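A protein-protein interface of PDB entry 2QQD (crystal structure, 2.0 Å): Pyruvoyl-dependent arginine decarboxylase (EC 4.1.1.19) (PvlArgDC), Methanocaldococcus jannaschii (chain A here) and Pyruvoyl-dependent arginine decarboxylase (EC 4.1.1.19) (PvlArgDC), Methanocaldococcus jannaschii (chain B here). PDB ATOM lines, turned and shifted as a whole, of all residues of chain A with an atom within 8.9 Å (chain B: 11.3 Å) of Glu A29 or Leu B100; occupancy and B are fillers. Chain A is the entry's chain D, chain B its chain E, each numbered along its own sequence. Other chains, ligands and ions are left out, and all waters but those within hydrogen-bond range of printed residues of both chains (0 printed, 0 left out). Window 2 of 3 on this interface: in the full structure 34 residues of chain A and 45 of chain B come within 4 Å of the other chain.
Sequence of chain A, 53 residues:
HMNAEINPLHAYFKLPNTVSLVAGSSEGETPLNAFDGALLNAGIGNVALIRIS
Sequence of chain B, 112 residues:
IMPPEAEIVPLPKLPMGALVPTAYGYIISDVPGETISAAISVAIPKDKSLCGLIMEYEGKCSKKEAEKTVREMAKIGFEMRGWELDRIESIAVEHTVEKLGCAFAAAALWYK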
ATOM      1  N   SER A  25      14.715 -11.358  26.177  1.00  0.00           N
ATOM      2  CA  SER A  25      13.911 -10.299  25.590  1.00  0.00           C
ATOM      3  C   SER A  25      14.404  -8.986  26.163  1.00  0.00           C
ATOM      4  O   SER A  25      15.189  -8.970  27.107  1.00  0.00           O
ATOM      5  CB  SER A  25      12.428 -10.495  25.924  1.00  0.00           C
ATOM      6  OG  SER A  25      12.216 -10.436  27.327  1.00  0.00           O
ATOM      7  N   SER A  26      13.935  -7.884  25.596  1.00  0.00           N
ATOM      8  CA  SER A  26      14.358  -6.582  26.065  1.00  0.00           C
ATOM      9  C   SER A  26      13.642  -5.456  25.349  1.00  0.00           C
ATOM     10  O   SER A  26      13.082  -5.634  24.266  1.00  0.00           O
ATOM     11  CB  SER A  26      15.868  -6.425  25.848  1.00  0.00           C
ATOM     12  OG  SER A  26      16.259  -5.069  25.947  1.00  0.00           O
ATOM     13  N   GLU A  27      13.661  -4.290  25.978  1.00  0.00           N
ATOM     14  CA  GLU A  27      13.070  -3.101  25.391  1.00  0.00           C
ATOM     15  C   GLU A  27      14.232  -2.406  24.686  1.00  0.00           C
ATOM     16  O   GLU A  27      15.395  -2.771  24.879  1.00  0.00           O
ATOM     17  CB  GLU A  27      12.501  -2.196  26.487  1.00  0.00           C
ATOM     18  CG  GLU A  27      11.247  -2.743  27.167  1.00  0.00           C
ATOM     19  CD  GLU A  27       9.970  -2.417  26.403  1.00  0.00           C
ATOM     20  OE1 GLU A  27       9.195  -3.357  26.103  1.00  0.00           O
ATOM     21  OE2 GLU A  27       9.736  -1.222  26.111  1.00  0.00           O
ATOM     22  N   GLY A  28      13.926  -1.418  23.862  1.00  0.00           N
ATOM     23  CA  GLY A  28      14.974  -0.695  23.166  1.00  0.00           C
ATOM     24  C   GLY A  28      14.407   0.588  22.607  1.00  0.00           C
ATOM     25  O   GLY A  28      13.197   0.688  22.415  1.00  0.00           O
ATOM     26  N   GLU A  29      15.269   1.563  22.341  1.00  0.00           N
ATOM     27  CA  GLU A  29      14.831   2.843  21.798  1.00  0.00           C
ATOM     28  C   GLU A  29      14.615   2.746  20.294  1.00  0.00           C
ATOM     29  O   GLU A  29      14.050   3.651  19.671  1.00  0.00           O
ATOM     30  CB  GLU A  29      15.861   3.924  22.110  1.00  0.00           C
ATOM     31  CG  GLU A  29      16.307   3.925  23.559  1.00  0.00           C
ATOM     32  CD  GLU A  29      16.996   5.212  23.956  1.00  0.00           C
ATOM     33  OE1 GLU A  29      17.739   5.205  24.962  1.00  0.00           O
ATOM     34  OE2 GLU A  29      16.785   6.233  23.264  1.00  0.00           O
ATOM     35  N   THR A  30      15.089   1.647  19.714  1.00  0.00           N
ATOM     36  CA  THR A  30      14.943   1.380  18.289  1.00  0.00           C
ATOM     37  C   THR A  30      14.801  -0.129  18.152  1.00  0.00           C
ATOM     38  O   THR A  30      15.144  -0.871  19.072  1.00  0.00           O
ATOM     39  CB  THR A  30      16.183   1.823  17.486  1.00  0.00           C
ATOM     40  OG1 THR A  30      17.276   0.926  17.749  1.00  0.00           O
ATOM     41  CG2 THR A  30      16.574   3.241  17.861  1.00  0.00           C
ATOM     42  N   PRO A  31      14.286  -0.607  17.009  1.00  0.00           N
ATOM     43  CA  PRO A  31      14.132  -2.055  16.831  1.00  0.00           C
ATOM     44  C   PRO A  31      15.468  -2.775  16.967  1.00  0.00           C
ATOM     45  O   PRO A  31      15.567  -3.776  17.672  1.00  0.00           O
ATOM     46  CB  PRO A  31      13.558  -2.173  15.424  1.00  0.00           C
ATOM     47  CG  PRO A  31      12.787  -0.886  15.267  1.00  0.00           C
ATOM     48  CD  PRO A  31      13.736   0.127  15.859  1.00  0.00           C
ATOM     49  N   LEU A  32      16.494  -2.262  16.295  1.00  0.00           N
ATOM     50  CA  LEU A  32      17.814  -2.886  16.359  1.00  0.00           C
ATOM     51  C   LEU A  32      18.349  -2.896  17.786  1.00  0.00           C
ATOM     52  O   LEU A  32      18.932  -3.886  18.223  1.00  0.00           O
ATOM     53  CB  LEU A  32      18.800  -2.166  15.430  1.00  0.00           C
ATOM     54  CG  LEU A  32      20.182  -2.828  15.313  1.00  0.00           C
ATOM     55  CD1 LEU A  32      20.012  -4.263  14.824  1.00  0.00           C
ATOM     56  CD2 LEU A  32      21.066  -2.047  14.357  1.00  0.00           C
ATOM     57  N   ASN A  33      18.148  -1.807  18.523  1.00  0.00           N
ATOM     58  CA  ASN A  33      18.627  -1.760  19.899  1.00  0.00           C
ATOM     59  C   ASN A  33      17.864  -2.732  20.785  1.00  0.00           C
ATOM     60  O   ASN A  33      18.434  -3.309  21.705  1.00  0.00           O
ATOM     61  CB  ASN A  33      18.534  -0.343  20.469  1.00  0.00           C
ATOM     62  CG  ASN A  33      19.636   0.563  19.948  1.00  0.00           C
ATOM     63  OD1 ASN A  33      20.833   0.261  20.087  1.00  0.00           O
ATOM     64  ND2 ASN A  33      19.245   1.676  19.344  1.00  0.00           N
ATOM     65  N   ALA A  34      16.573  -2.910  20.518  1.00  0.00           N
ATOM     66  CA  ALA A  34      15.774  -3.845  21.303  1.00  0.00           C
ATOM     67  C   ALA A  34      16.308  -5.251  21.033  1.00  0.00           C
ATOM     68  O   ALA A  34      16.499  -6.043  21.958  1.00  0.00           O
ATOM     69  CB  ALA A  34      14.297  -3.755  20.894  1.00  0.00           C
ATOM     70  N   PHE A  35      16.541  -5.547  19.756  1.00  0.00           N
ATOM     71  CA  PHE A  35      17.065  -6.844  19.333  1.00  0.00           C
ATOM     72  C   PHE A  35      18.402  -7.106  20.059  1.00  0.00           C
ATOM     73  O   PHE A  35      18.610  -8.176  20.638  1.00  0.00           O
ATOM     74  CB  PHE A  35      17.276  -6.828  17.817  1.00  0.00           C
ATOM     75  CG  PHE A  35      17.778  -8.126  17.251  1.00  0.00           C
ATOM     76  CD1 PHE A  35      16.917  -9.210  17.088  1.00  0.00           C
ATOM     77  CD2 PHE A  35      19.108  -8.264  16.877  1.00  0.00           C
ATOM     78  CE1 PHE A  35      17.376 -10.417  16.556  1.00  0.00           C
ATOM     79  CE2 PHE A  35      19.582  -9.468  16.345  1.00  0.00           C
ATOM     80  CZ  PHE A  35      18.709 -10.548  16.183  1.00  0.00           C
ATOM     81  N   GLY A  37      19.473  -5.829  22.809  1.00  0.00           N
ATOM     82  CA  GLY A  37      19.230  -6.045  24.226  1.00  0.00           C
ATOM     83  C   GLY A  37      18.768  -7.460  24.528  1.00  0.00           C
ATOM     84  O   GLY A  37      19.132  -8.043  25.555  1.00  0.00           O
ATOM     85  N   TYR B  26      12.724 -14.386  16.295  1.00  0.00           N
ATOM     86  CA  TYR B  26      12.532 -13.207  17.109  1.00  0.00           C
ATOM     87  C   TYR B  26      11.340 -12.456  16.552  1.00  0.00           C
ATOM     88  O   TYR B  26      10.916 -12.688  15.416  1.00  0.00           O
ATOM     89  CB  TYR B  26      13.774 -12.319  17.057  1.00  0.00           C
ATOM     90  CG  TYR B  26      13.923 -11.584  15.751  1.00  0.00           C
ATOM     91  CD1 TYR B  26      13.534 -10.246  15.632  1.00  0.00           C
ATOM     92  CD2 TYR B  26      14.402 -12.235  14.617  1.00  0.00           C
ATOM     93  CE1 TYR B  26      13.622  -9.576  14.410  1.00  0.00           C
ATOM     94  CE2 TYR B  26      14.491 -11.580  13.395  1.00  0.00           C
ATOM     95  CZ  TYR B  26      14.099 -10.251  13.300  1.00  0.00           C
ATOM     96  OH  TYR B  26      14.197  -9.602  12.093  1.00  0.00           O
ATOM     97  N   ILE B  27      10.809 -11.557  17.365  1.00  0.00           N
ATOM     98  CA  ILE B  27       9.680 -10.734  16.983  1.00  0.00           C
ATOM     99  C   ILE B  27       9.849  -9.424  17.732  1.00  0.00           C
ATOM    100  O   ILE B  27      10.204  -9.417  18.913  1.00  0.00           O
ATOM    101  CB  ILE B  27       8.336 -11.405  17.368  1.00  0.00           C
ATOM    102  CG1 ILE B  27       7.168 -10.460  17.054  1.00  0.00           C
ATOM    103  CG2 ILE B  27       8.339 -11.780  18.844  1.00  0.00           C
ATOM    104  CD1 ILE B  27       5.803 -11.125  17.157  1.00  0.00           C
ATOM    105  N   ILE B  28       9.636  -8.319  17.024  1.00  0.00           N
ATOM    106  CA  ILE B  28       9.752  -6.996  17.614  1.00  0.00           C
ATOM    107  C   ILE B  28       8.386  -6.316  17.523  1.00  0.00           C
ATOM    108  O   ILE B  28       7.724  -6.386  16.492  1.00  0.00           O
ATOM    109  CB  ILE B  28      10.807  -6.153  16.868  1.00  0.00           C
ATOM    110  CG1 ILE B  28      12.162  -6.875  16.910  1.00  0.00           C
ATOM    111  CG2 ILE B  28      10.930  -4.768  17.512  1.00  0.00           C
ATOM    112  CD1 ILE B  28      13.280  -6.149  16.203  1.00  0.00           C
ATOM    113  N   SER B  29       7.964  -5.675  18.606  1.00  0.00           N
ATOM    114  CA  SER B  29       6.672  -4.996  18.628  1.00  0.00           C
ATOM    115  C   SER B  29       6.746  -3.655  19.330  1.00  0.00           C
ATOM    116  O   SER B  29       7.396  -3.525  20.365  1.00  0.00           O
ATOM    117  CB  SER B  29       5.627  -5.864  19.326  1.00  0.00           C
ATOM    118  OG  SER B  29       4.418  -5.147  19.518  1.00  0.00           O
ATOM    119  N   ASP B  30       6.074  -2.659  18.760  1.00  0.00           N
ATOM    120  CA  ASP B  30       6.040  -1.321  19.337  1.00  0.00           C
ATOM    121  C   ASP B  30       4.627  -0.959  19.784  1.00  0.00           C
ATOM    122  O   ASP B  30       4.244   0.208  19.765  1.00  0.00           O
ATOM    123  CB  ASP B  30       6.528  -0.279  18.327  1.00  0.00           C
ATOM    124  CG  ASP B  30       5.728  -0.291  17.036  1.00  0.00           C
ATOM    125  OD1 ASP B  30       4.591  -0.806  17.035  1.00  0.00           O
ATOM    126  OD2 ASP B  30       6.232   0.227  16.019  1.00  0.00           O
ATOM    127  N   VAL B  31       3.851  -1.968  20.168  1.00  0.00           N
ATOM    128  CA  VAL B  31       2.485  -1.751  20.633  1.00  0.00           C
ATOM    129  C   VAL B  31       2.469  -1.964  22.137  1.00  0.00           C
ATOM    130  O   VAL B  31       2.616  -3.086  22.611  1.00  0.00           O
ATOM    131  CB  VAL B  31       1.496  -2.745  19.991  1.00  0.00           C
ATOM    132  CG1 VAL B  31       0.101  -2.521  20.559  1.00  0.00           C
ATOM    133  CG2 VAL B  31       1.486  -2.575  18.480  1.00  0.00           C
ATOM    134  N   PRO B  32       2.283  -0.884  22.910  1.00  0.00           N
ATOM    135  CA  PRO B  32       2.254  -0.963  24.374  1.00  0.00           C
ATOM    136  C   PRO B  32       1.360  -2.072  24.925  1.00  0.00           C
ATOM    137  O   PRO B  32       0.293  -2.353  24.384  1.00  0.00           O
ATOM    138  CB  PRO B  32       1.768   0.424  24.782  1.00  0.00           C
ATOM    139  CG  PRO B  32       2.308   1.299  23.692  1.00  0.00           C
ATOM    140  CD  PRO B  32       1.997   0.488  22.458  1.00  0.00           C
ATOM    141  N   GLY B  33       1.813  -2.703  26.001  1.00  0.00           N
ATOM    142  CA  GLY B  33       1.038  -3.758  26.627  1.00  0.00           C
ATOM    143  C   GLY B  33       0.961  -5.077  25.884  1.00  0.00           C
ATOM    144  O   GLY B  33       0.679  -6.110  26.497  1.00  0.00           O
ATOM    145  N   GLU B  34       1.202  -5.061  24.577  1.00  0.00           N
ATOM    146  CA  GLU B  34       1.147  -6.292  23.793  1.00  0.00           C
ATOM    147  C   GLU B  34       2.161  -7.340  24.255  1.00  0.00           C
ATOM    148  O   GLU B  34       3.284  -7.012  24.648  1.00  0.00           O
ATOM    149  CB  GLU B  34       1.364  -5.992  22.312  1.00  0.00           C
ATOM    150  CG  GLU B  34       1.373  -7.235  21.449  1.00  0.00           C
ATOM    151  CD  GLU B  34       1.172  -6.932  19.981  1.00  0.00           C
ATOM    152  OE1 GLU B  34       1.951  -6.132  19.421  1.00  0.00           O
ATOM    153  OE2 GLU B  34       0.232  -7.501  19.385  1.00  0.00           O
ATOM    154  N   THR B  35       1.753  -8.604  24.214  1.00  0.00           N
ATOM    155  CA  THR B  35       2.620  -9.702  24.617  1.00  0.00           C
ATOM    156  C   THR B  35       3.164 -10.378  23.369  1.00  0.00           C
ATOM    157  O   THR B  35       2.433 -10.577  22.401  1.00  0.00           O
ATOM    158  CB  THR B  35       1.857 -10.752  25.461  1.00  0.00           C
ATOM    159  OG1 THR B  35       1.479 -10.175  26.716  1.00  0.00           O
ATOM    160  CG2 THR B  35       2.736 -11.975  25.720  1.00  0.00           C
ATOM    161  N   ILE B  36       4.448 -10.718  23.388  1.00  0.00           N
ATOM    162  CA  ILE B  36       5.066 -11.377  22.244  1.00  0.00           C
ATOM    163  C   ILE B  36       5.990 -12.474  22.733  1.00  0.00           C
ATOM    164  O   ILE B  36       6.617 -12.345  23.781  1.00  0.00           O
ATOM    165  CB  ILE B  36       5.859 -10.373  21.370  1.00  0.00           C
ATOM    166  CG1 ILE B  36       6.963  -9.704  22.202  1.00  0.00           C
ATOM    167  CG2 ILE B  36       4.907  -9.332  20.791  1.00  0.00           C
ATOM    168  CD1 ILE B  36       7.731  -8.627  21.456  1.00  0.00           C
ATOM    169  N   LYS B  60       2.490 -13.348  18.524  1.00  0.00           N
ATOM    170  CA  LYS B  60       1.818 -12.642  19.602  1.00  0.00           C
ATOM    171  C   LYS B  60       1.002 -13.620  20.434  1.00  0.00           C
ATOM    172  O   LYS B  60      -0.203 -13.768  20.242  1.00  0.00           O
ATOM    173  CB  LYS B  60       0.934 -11.550  19.007  1.00  0.00           C
ATOM    174  CG  LYS B  60       1.747 -10.509  18.253  1.00  0.00           C
ATOM    175  CD  LYS B  60       0.907  -9.686  17.300  1.00  0.00           C
ATOM    176  CE  LYS B  60       1.797  -8.797  16.443  1.00  0.00           C
ATOM    177  NZ  LYS B  60       1.042  -8.152  15.337  1.00  0.00           N
ATOM    178  N   HIS B  95       7.577 -11.564  26.266  1.00  0.00           N
ATOM    179  CA  HIS B  95       7.836 -10.203  26.699  1.00  0.00           C
ATOM    180  C   HIS B  95       6.578  -9.355  26.558  1.00  0.00           C
ATOM    181  O   HIS B  95       5.899  -9.405  25.531  1.00  0.00           O
ATOM    182  CB  HIS B  95       8.946  -9.607  25.832  1.00  0.00           C
ATOM    183  CG  HIS B  95       9.298  -8.195  26.175  1.00  0.00           C
ATOM    184  ND1 HIS B  95      10.251  -7.873  27.115  1.00  0.00           N
ATOM    185  CD2 HIS B  95       8.826  -7.019  25.698  1.00  0.00           C
ATOM    186  CE1 HIS B  95      10.355  -6.558  27.202  1.00  0.00           C
ATOM    187  NE2 HIS B  95       9.502  -6.017  26.351  1.00  0.00           N
ATOM    188  N   THR B  96       6.260  -8.585  27.592  1.00  0.00           N
ATOM    189  CA  THR B  96       5.102  -7.706  27.534  1.00  0.00           C
ATOM    190  C   THR B  96       5.654  -6.332  27.177  1.00  0.00           C
ATOM    191  O   THR B  96       6.327  -5.695  27.983  1.00  0.00           O
ATOM    192  CB  THR B  96       4.360  -7.622  28.886  1.00  0.00           C
ATOM    193  OG1 THR B  96       4.016  -8.942  29.334  1.00  0.00           O
ATOM    194  CG2 THR B  96       3.086  -6.805  28.728  1.00  0.00           C
ATOM    195  N   VAL B  97       5.369  -5.889  25.961  1.00  0.00           N
ATOM    196  CA  VAL B  97       5.853  -4.612  25.459  1.00  0.00           C
ATOM    197  C   VAL B  97       5.469  -3.391  26.287  1.00  0.00           C
ATOM    198  O   VAL B  97       4.317  -3.240  26.700  1.00  0.00           O
ATOM    199  CB  VAL B  97       5.367  -4.384  24.012  1.00  0.00           C
ATOM    200  CG1 VAL B  97       5.870  -3.035  23.490  1.00  0.00           C
ATOM    201  CG2 VAL B  97       5.847  -5.525  23.119  1.00  0.00           C
ATOM    202  N   GLU B  98       6.451  -2.525  26.529  1.00  0.00           N
ATOM    203  CA  GLU B  98       6.222  -1.285  27.263  1.00  0.00           C
ATOM    204  C   GLU B  98       6.068  -0.237  26.174  1.00  0.00           C
ATOM    205  O   GLU B  98       5.007   0.361  26.014  1.00  0.00           O
ATOM    206  CB  GLU B  98       7.420  -0.928  28.142  1.00  0.00           C
ATOM    207  CG  GLU B  98       7.695  -1.889  29.277  1.00  0.00           C
ATOM    208  CD  GLU B  98       8.872  -1.443  30.131  1.00  0.00           C
ATOM    209  OE1 GLU B  98       8.783  -0.363  30.756  1.00  0.00           O
ATOM    210  OE2 GLU B  98       9.891  -2.171  30.174  1.00  0.00           O
ATOM    211  N   LYS B  99       7.138  -0.035  25.415  1.00  0.00           N
ATOM    212  CA  LYS B  99       7.130   0.917  24.312  1.00  0.00           C
ATOM    213  C   LYS B  99       7.625   0.226  23.042  1.00  0.00           C
ATOM    214  O   LYS B  99       7.021   0.346  21.978  1.00  0.00           O
ATOM    215  CB  LYS B  99       8.018   2.115  24.644  1.00  0.00           C
ATOM    216  CG  LYS B  99       7.675   2.771  25.975  1.00  0.00           C
ATOM    217  CD  LYS B  99       8.563   3.974  26.245  1.00  0.00           C
ATOM    218  CE  LYS B  99       8.234   5.107  25.292  1.00  0.00           C
ATOM    219  NZ  LYS B  99       6.802   5.499  25.420  1.00  0.00           N
ATOM    220  N   LEU B 100       8.727  -0.506  23.165  1.00  0.00           N
ATOM    221  CA  LEU B 100       9.298  -1.230  22.037  1.00  0.00           C
ATOM    222  C   LEU B 100      10.130  -2.388  22.577  1.00  0.00           C
ATOM    223  O   LEU B 100      11.196  -2.186  23.152  1.00  0.00           O
ATOM    224  CB  LEU B 100      10.164  -0.291  21.190  1.00  0.00           C
ATOM    225  CG  LEU B 100      10.963  -0.888  20.021  1.00  0.00           C
ATOM    226  CD1 LEU B 100      10.036  -1.613  19.054  1.00  0.00           C
ATOM    227  CD2 LEU B 100      11.714   0.229  19.310  1.00  0.00           C
ATOM    228  N   GLY B 101       9.635  -3.605  22.397  1.00  0.00           N
ATOM    229  CA  GLY B 101      10.358  -4.753  22.903  1.00  0.00           C
ATOM    230  C   GLY B 101      10.621  -5.820  21.865  1.00  0.00           C
ATOM    231  O   GLY B 101      10.042  -5.813  20.778  1.00  0.00           O
ATOM    232  N   CYS B 102      11.508  -6.744  22.211  1.00  0.00           N
ATOM    233  CA  CYS B 102      11.851  -7.840  21.325  1.00  0.00           C
ATOM    234  C   CYS B 102      11.955  -9.133  22.117  1.00  0.00           C
ATOM    235  O   CYS B 102      12.540  -9.159  23.200  1.00  0.00           O
ATOM    236  CB  CYS B 102      13.187  -7.565  20.622  1.00  0.00           C
ATOM    237  SG  CYS B 102      13.923  -9.056  19.878  1.00  0.00           S
ATOM    238  N   ALA B 103      11.366 -10.195  21.573  1.00  0.00           N
ATOM    239  CA  ALA B 103      11.409 -11.522  22.177  1.00  0.00           C
ATOM    240  C   ALA B 103      12.346 -12.317  21.270  1.00  0.00           C
ATOM    241  O   ALA B 103      12.188 -12.293  20.056  1.00  0.00           O
ATOM    242  CB  ALA B 103      10.026 -12.146  22.179  1.00  0.00           C
ATOM    243  N   PHE B 104      13.296 -13.037  21.859  1.00  0.00           N
ATOM    244  CA  PHE B 104      14.285 -13.774  21.072  1.00  0.00           C
ATOM    245  C   PHE B 104      14.596 -15.183  21.596  1.00  0.00           C
ATOM    246  O   PHE B 104      14.760 -15.387  22.797  1.00  0.00           O
ATOM    247  CB  PHE B 104      15.564 -12.923  21.039  1.00  0.00           C
ATOM    248  CG  PHE B 104      16.736 -13.590  20.395  1.00  0.00           C
ATOM    249  CD1 PHE B 104      16.855 -13.638  19.010  1.00  0.00           C
ATOM    250  CD2 PHE B 104      17.741 -14.149  21.175  1.00  0.00           C
ATOM    251  CE1 PHE B 104      17.970 -14.229  18.410  1.00  0.00           C
ATOM    252  CE2 PHE B 104      18.855 -14.742  20.586  1.00  0.00           C
ATOM    253  CZ  PHE B 104      18.969 -14.780  19.201  1.00  0.00           C
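The side-chain hydroxyl (OG) of Ser A25 sits at hydrogen-bond distance from a ring nitrogen (ND1) of His B95, at 3.2 Å. N of Cys B102 sits at hydrogen-bond distance from O of Ser A26 (2.8 Å). NE2 of His B95 is in hydrogen-bond range of OE1 of Glu A27 (2.7 Å). The side-chain carboxylate of Glu A27 lies within hydrogen-bond range of the backbone NH of Glu B98 (2.9 Å). The side-chain carboxylate (OE2) of Glu A27 sits at hydrogen-bond distance from the backbone NH (N) of Lys B99 (2.9 Å). The side-chain carboxylate (OE2) of Glu A27 sits at hydrogen-bond distance from the backbone NH (N) of Leu B100, 3.2 Å away. The backbone NH of Gly A28 lies within hydrogen-bond range of the backbone carbonyl oxygen of Leu B100 (2.9 Å).
O of Cys B102 touches CA of Ser A25, at 3.0 Å. His B95 touches Ser A26. Ser A26 touches Gly B101. Glu A27 touches Val B97. Gly B101 touches Glu A27. CD2 of Leu B100 touches C of Glu A29 (3.96 Å). Thr A30 touches Leu B100 (C to CD2, 3.3 Å). Ala A34 touches Cys B102 (O to CB, 3.9 Å). Tyr B26 touches Phe A35. CA of Phe A35 touches SG of Cys B102, 3.9 Å away.
OG1 of Thr A30 lies within hydrogen-bond range of ND2 of Asn A33 (2.6 Å). N of Ser B29 lies within hydrogen-bond range of O of Gly B101 (3.0 Å). The backbone NH (N) of Gly B33 sits at hydrogen-bond distance from the backbone carbonyl oxygen (O) of Val B97 (2.7 Å). O of Glu B34 is in hydrogen-bond range of N of Val B97, at 2.7 Å. O of Ile B36 is in hydrogen-bond range of N of His B95, at 2.8 Å.
Of chain B, only Leu B100 comes within 4 Å of Glu A29. Leu B100 touches just these residues of chain A: Glu A27, Gly A28, Glu A29, Thr A30 and Pro A31. Glu A27 touches just these residues of chain B: His B95 (2.7 Å), Val B97 (3.6 Å), Glu B98 (2.9 Å), Lys B99 (2.9 Å), Leu B100 (3.1 Å) and Gly B101 (3.7 Å). Of chain B, only Ile B28 and Leu B100 come within 4 Å of Pro A31. Printed residues of chain A within 4 Å of Tyr B26: Phe A35 (3.7 Å). Of the printed residues of chain B, Phe A35 touches Tyr B26 and Cys B102. Printed residues of chain A within 4 Å of Lys B99: Glu A27 (2.9 Å). Leu A32 touches none of the printed residues of chain B. The nearest residue of chain B that does not touch Glu A29 is Lys B99 (7.4 Å). The nearest residue of chain A that does not touch Leu B100 is Ser A26 (4.1 Å).
Printed residues of chain A that touch a printed residue of chain B: Ser A25, Ser A26, Glu A27, Gly A28, Glu A29, Thr A30, Pro A31, Ala A34 and Phe A35. Along chain A the printed residues that touch a printed residue of chain B span positions 25 to 35. Of the 22 printed residues of chain B, 9 touch a printed residue of chain A. Among the printed residues, 19 pairs touch across the chains.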
